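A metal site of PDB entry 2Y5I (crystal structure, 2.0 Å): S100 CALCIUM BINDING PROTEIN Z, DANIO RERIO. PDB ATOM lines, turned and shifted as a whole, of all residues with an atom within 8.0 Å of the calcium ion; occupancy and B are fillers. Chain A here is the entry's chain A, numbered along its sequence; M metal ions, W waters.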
ATOM      1  N   PHE A  16      -2.051   0.397   0.670  1.00  0.00           N
ATOM      2  CA  PHE A  16      -1.135   1.334   1.321  1.00  0.00           C
ATOM      3  C   PHE A  16      -0.552   0.746   2.590  1.00  0.00           C
ATOM      4  O   PHE A  16       0.682   0.700   2.799  1.00  0.00           O
ATOM      5  CB  PHE A  16      -1.841   2.646   1.636  1.00  0.00           C
ATOM      6  CG  PHE A  16      -0.942   3.692   2.267  1.00  0.00           C
ATOM      7  CD1 PHE A  16      -0.104   4.473   1.478  1.00  0.00           C
ATOM      8  CD2 PHE A  16      -0.922   3.897   3.632  1.00  0.00           C
ATOM      9  CE1 PHE A  16       0.695   5.454   2.035  1.00  0.00           C
ATOM     10  CE2 PHE A  16      -0.154   4.896   4.177  1.00  0.00           C
ATOM     11  CZ  PHE A  16       0.648   5.656   3.395  1.00  0.00           C
ATOM     12  N   TYR A  19       2.175  -2.038   2.719  1.00  0.00           N
ATOM     13  CA  TYR A  19       3.589  -1.689   2.511  1.00  0.00           C
ATOM     14  C   TYR A  19       4.144  -0.649   3.488  1.00  0.00           C
ATOM     15  O   TYR A  19       5.349  -0.532   3.611  1.00  0.00           O
ATOM     16  CB  TYR A  19       3.835  -1.179   1.059  1.00  0.00           C
ATOM     17  CG  TYR A  19       3.471  -2.200   0.009  1.00  0.00           C
ATOM     18  CD1 TYR A  19       4.401  -3.149  -0.416  1.00  0.00           C
ATOM     19  CD2 TYR A  19       2.173  -2.251  -0.520  1.00  0.00           C
ATOM     20  CE1 TYR A  19       4.047  -4.100  -1.371  1.00  0.00           C
ATOM     21  CE2 TYR A  19       1.793  -3.215  -1.439  1.00  0.00           C
ATOM     22  CZ  TYR A  19       2.722  -4.122  -1.872  1.00  0.00           C
ATOM     23  OH  TYR A  19       2.353  -5.048  -2.791  1.00  0.00           O
ATOM     24  N   SER A  20       3.279   0.167   4.116  1.00  0.00           N
ATOM     25  CA  SER A  20       3.727   1.330   4.909  1.00  0.00           C
ATOM     26  C   SER A  20       4.235   0.971   6.302  1.00  0.00           C
ATOM     27  O   SER A  20       4.891   1.795   6.985  1.00  0.00           O
ATOM     28  CB  SER A  20       2.587   2.359   5.038  1.00  0.00           C
ATOM     29  OG  SER A  20       1.527   1.869   5.896  1.00  0.00           O
ATOM     30  N   GLY A  21       3.946  -0.256   6.753  1.00  0.00           N
ATOM     31  CA  GLY A  21       4.257  -0.663   8.095  1.00  0.00           C
ATOM     32  C   GLY A  21       5.528  -1.489   8.309  1.00  0.00           C
ATOM     33  O   GLY A  21       5.705  -2.098   9.340  1.00  0.00           O
ATOM     34  N   SER A  22       6.418  -1.554   7.311  1.00  0.00           N
ATOM     35  CA  SER A  22       7.653  -2.287   7.487  1.00  0.00           C
ATOM     36  C   SER A  22       8.668  -1.543   8.330  1.00  0.00           C
ATOM     37  O   SER A  22       9.435  -2.163   9.082  1.00  0.00           O
ATOM     38  CB  SER A  22       8.292  -2.552   6.133  1.00  0.00           C
ATOM     39  OG  SER A  22       7.431  -3.402   5.433  1.00  0.00           O
ATOM     40  N   GLU A  23       8.668  -0.224   8.207  1.00  0.00           N
ATOM     41  CA  GLU A  23       9.675   0.574   8.911  1.00  0.00           C
ATOM     42  C   GLU A  23       9.214   2.003   9.085  1.00  0.00           C
ATOM     43  O   GLU A  23       8.294   2.490   8.390  1.00  0.00           O
ATOM     44  CB  GLU A  23      11.031   0.575   8.171  1.00  0.00           C
ATOM     45  CG  GLU A  23      10.974   1.264   6.798  1.00  0.00           C
ATOM     46  CD  GLU A  23      12.295   1.264   6.004  1.00  0.00           C
ATOM     47  OE1 GLU A  23      13.332   0.900   6.516  1.00  0.00           O
ATOM     48  OE2 GLU A  23      12.289   1.659   4.828  1.00  0.00           O
ATOM     49  N   GLY A  24       9.905   2.693   9.978  1.00  0.00           N
ATOM     50  CA  GLY A  24       9.592   4.080  10.239  1.00  0.00           C
ATOM     51  C   GLY A  24       8.132   4.243  10.582  1.00  0.00           C
ATOM     52  O   GLY A  24       7.498   3.353  11.112  1.00  0.00           O
ATOM     53  N   ASP A  25       7.591   5.414  10.295  1.00  0.00           N
ATOM     54  CA  ASP A  25       6.156   5.642  10.493  1.00  0.00           C
ATOM     55  C   ASP A  25       5.329   4.503   9.870  1.00  0.00           C
ATOM     56  O   ASP A  25       5.466   4.182   8.709  1.00  0.00           O
ATOM     57  CB  ASP A  25       5.715   6.991   9.886  1.00  0.00           C
ATOM     58  CG  ASP A  25       4.332   7.465  10.406  1.00  0.00           C
ATOM     59  OD1 ASP A  25       3.312   6.724  10.366  1.00  0.00           O
ATOM     60  OD2 ASP A  25       4.246   8.623  10.899  1.00  0.00           O
ATOM     61  N   LYS A  26       4.431   3.967  10.657  1.00  0.00           N
ATOM     62  CA  LYS A  26       3.602   2.850  10.263  1.00  0.00           C
ATOM     63  C   LYS A  26       2.584   3.260   9.164  1.00  0.00           C
ATOM     64  O   LYS A  26       2.103   2.428   8.379  1.00  0.00           O
ATOM     65  CB  LYS A  26       2.928   2.325  11.555  1.00  0.00           C
ATOM     66  CG  LYS A  26       1.990   1.124  11.375  1.00  0.00           C
ATOM     67  CD  LYS A  26       1.320   0.546  12.663  1.00  0.00           C
ATOM     68  CE  LYS A  26       0.868  -0.958  12.332  1.00  0.00           C
ATOM     69  NZ  LYS A  26       0.225  -1.855  13.399  1.00  0.00           N
ATOM     70  N   TYR A  27       2.283   4.550   9.108  1.00  0.00           N
ATOM     71  CA  TYR A  27       1.291   5.109   8.208  1.00  0.00           C
ATOM     72  C   TYR A  27       1.865   6.005   7.126  1.00  0.00           C
ATOM     73  O   TYR A  27       1.148   6.757   6.514  1.00  0.00           O
ATOM     74  CB  TYR A  27       0.246   5.893   9.009  1.00  0.00           C
ATOM     75  CG  TYR A  27      -0.417   5.105  10.128  1.00  0.00           C
ATOM     76  CD1 TYR A  27      -0.631   3.742  10.040  1.00  0.00           C
ATOM     77  CD2 TYR A  27      -0.902   5.753  11.234  1.00  0.00           C
ATOM     78  CE1 TYR A  27      -1.277   3.063  11.059  1.00  0.00           C
ATOM     79  CE2 TYR A  27      -1.524   5.088  12.249  1.00  0.00           C
ATOM     80  CZ  TYR A  27      -1.700   3.745  12.164  1.00  0.00           C
ATOM     81  OH  TYR A  27      -2.352   3.110  13.197  1.00  0.00           O
ATOM     82  N   LYS A  28       3.174   5.926   6.895  1.00  0.00           N
ATOM     83  CA  LYS A  28       3.783   6.563   5.727  1.00  0.00           C
ATOM     84  C   LYS A  28       4.713   5.593   5.023  1.00  0.00           C
ATOM     85  O   LYS A  28       5.343   4.710   5.646  1.00  0.00           O
ATOM     86  CB  LYS A  28       4.553   7.811   6.123  1.00  0.00           C
ATOM     87  CG  LYS A  28       3.771   8.864   6.902  1.00  0.00           C
ATOM     88  CD  LYS A  28       4.672  10.045   7.171  1.00  0.00           C
ATOM     89  CE  LYS A  28       4.080  11.107   8.061  1.00  0.00           C
ATOM     90  NZ  LYS A  28       5.206  12.057   8.511  1.00  0.00           N
ATOM     91  N   LEU A  29       4.863   5.819   3.719  1.00  0.00           N
ATOM     92  CA  LEU A  29       5.782   5.039   2.926  1.00  0.00           C
ATOM     93  C   LEU A  29       7.170   5.676   2.845  1.00  0.00           C
ATOM     94  O   LEU A  29       7.326   6.816   2.387  1.00  0.00           O
ATOM     95  CB  LEU A  29       5.234   4.848   1.518  1.00  0.00           C
ATOM     96  CG  LEU A  29       3.898   4.144   1.326  1.00  0.00           C
ATOM     97  CD1 LEU A  29       3.329   4.500  -0.053  1.00  0.00           C
ATOM     98  CD2 LEU A  29       4.081   2.628   1.467  1.00  0.00           C
ATOM     99  N   SER A  30       8.187   4.902   3.222  1.00  0.00           N
ATOM    100  CA  SER A  30       9.572   5.279   2.951  1.00  0.00           C
ATOM    101  C   SER A  30       9.805   5.087   1.468  1.00  0.00           C
ATOM    102  O   SER A  30       9.002   4.460   0.831  1.00  0.00           O
ATOM    103  CB  SER A  30      10.532   4.376   3.724  1.00  0.00           C
ATOM    104  OG  SER A  30      10.345   3.036   3.241  1.00  0.00           O
ATOM    105  N   LYS A  31      10.904   5.617   0.942  1.00  0.00           N
ATOM    106  CA  LYS A  31      11.323   5.331  -0.456  1.00  0.00           C
ATOM    107  C   LYS A  31      11.344   3.808  -0.710  1.00  0.00           C
ATOM    108  O   LYS A  31      10.893   3.351  -1.715  1.00  0.00           O
ATOM    109  CB  LYS A  31      12.701   5.897  -0.714  1.00  0.00           C
ATOM    110  CG  LYS A  31      13.225   5.872  -2.160  1.00  0.00           C
ATOM    111  CD  LYS A  31      14.699   6.070  -2.083  1.00  0.00           C
ATOM    112  CE  LYS A  31      15.369   6.305  -3.361  1.00  0.00           C
ATOM    113  NZ  LYS A  31      16.773   6.719  -3.121  1.00  0.00           N
ATOM    114  N   GLU A  33       9.704   1.322   0.865  1.00  0.00           N
ATOM    115  CA  GLU A  33       8.339   0.824   0.877  1.00  0.00           C
ATOM    116  C   GLU A  33       7.563   1.227  -0.400  1.00  0.00           C
ATOM    117  O   GLU A  33       6.839   0.412  -0.975  1.00  0.00           O
ATOM    118  CB  GLU A  33       7.633   1.305   2.147  1.00  0.00           C
ATOM    119  CG  GLU A  33       8.149   0.705   3.461  1.00  0.00           C
ATOM    120  CD  GLU A  33       7.575   1.357   4.722  1.00  0.00           C
ATOM    121  OE1 GLU A  33       7.181   2.548   4.660  1.00  0.00           O
ATOM    122  OE2 GLU A  33       7.510   0.712   5.806  1.00  0.00           O
ATOM    123  N   LEU A  34       7.727   2.479  -0.822  1.00  0.00           N
ATOM    124  CA  LEU A  34       7.175   2.965  -2.063  1.00  0.00           C
ATOM    125  C   LEU A  34       7.670   2.117  -3.246  1.00  0.00           C
ATOM    126  O   LEU A  34       6.869   1.687  -4.056  1.00  0.00           O
ATOM    127  CB  LEU A  34       7.527   4.445  -2.287  1.00  0.00           C
ATOM    128  CG  LEU A  34       6.988   5.072  -3.594  1.00  0.00           C
ATOM    129  CD1 LEU A  34       5.419   5.099  -3.667  1.00  0.00           C
ATOM    130  CD2 LEU A  34       7.617   6.432  -3.858  1.00  0.00           C
ATOM    131  N   GLU A  69       8.876  11.056   3.255  1.00  0.00           N
ATOM    132  CA  GLU A  69       7.889   9.952   3.247  1.00  0.00           C
ATOM    133  C   GLU A  69       6.777  10.306   2.310  1.00  0.00           C
ATOM    134  O   GLU A  69       6.555  11.490   2.003  1.00  0.00           O
ATOM    135  CB  GLU A  69       7.237   9.785   4.608  1.00  0.00           C
ATOM    136  CG  GLU A  69       8.163   9.764   5.752  1.00  0.00           C
ATOM    137  CD  GLU A  69       8.774   8.429   5.991  1.00  0.00           C
ATOM    138  OE1 GLU A  69       8.128   7.405   5.715  1.00  0.00           O
ATOM    139  OE2 GLU A  69       9.903   8.392   6.502  1.00  0.00           O
ATOM    140  N   VAL A  70       6.050   9.273   1.887  1.00  0.00           N
ATOM    141  CA  VAL A  70       4.832   9.439   1.126  1.00  0.00           C
ATOM    142  C   VAL A  70       3.692   9.014   2.058  1.00  0.00           C
ATOM    143  O   VAL A  70       3.456   7.813   2.304  1.00  0.00           O
ATOM    144  CB  VAL A  70       4.845   8.592  -0.152  1.00  0.00           C
ATOM    145  CG1 VAL A  70       3.465   8.574  -0.836  1.00  0.00           C
ATOM    146  CG2 VAL A  70       5.937   9.093  -1.151  1.00  0.00           C
HETATM  147 CA    CA M   1       6.709   3.205   6.854  1.00  0.00          CA
HETATM  148  O   HOH W   1       8.288   4.962   6.697  1.00  0.00           O
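The calcium ion is bound by the backbone carbonyl oxygen (O) of Ser 20 (2.3 Å).
The calcium ion is bound by O of Glu 23, 2.3 Å away.
OE1 of Glu 33 is bound to the calcium ion.
O of Lys 28 binds the calcium ion.
The calcium ion is bound by water W1 (2.4 Å).
The calcium ion is bound by the backbone carbonyl oxygen (O) of Asp 25 (2.4 Å).
OE2 of Glu 33 is bound to the calcium ion.
The calcium ion has seven donor atoms within binding distance.
The backbone carbonyl oxygen of Lys 26 lies within hydrogen-bond range of the side-chain hydroxyl of Ser 20 (2.6 Å).
The backbone carbonyl oxygen (O) of Phe 16 lies close to the side-chain hydroxyl (OG) of Ser 20 (3.4 Å).
OE2 of Glu 23 is in hydrogen-bond range of OG of Ser 30.
N of Glu 33 sits at hydrogen-bond distance from OG of Ser 30, 3.0 Å away.
The side-chain carboxylate of Glu 33 sits close to the backbone NH of Ser 22 (2.9 Å).
OD1 of Asp 25 sits at hydrogen-bond distance from N of Tyr 27 (2.7 Å).
Water W1 bridges OE1 of Glu 69 (2.6 Å) and N of Ser 30 (3.5 Å).
Of the 18 residues printed, 5 come within 4 Å of the calcium ion.
Along chain A the residues within 4 Å of the calcium ion span positions 20 to 33.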
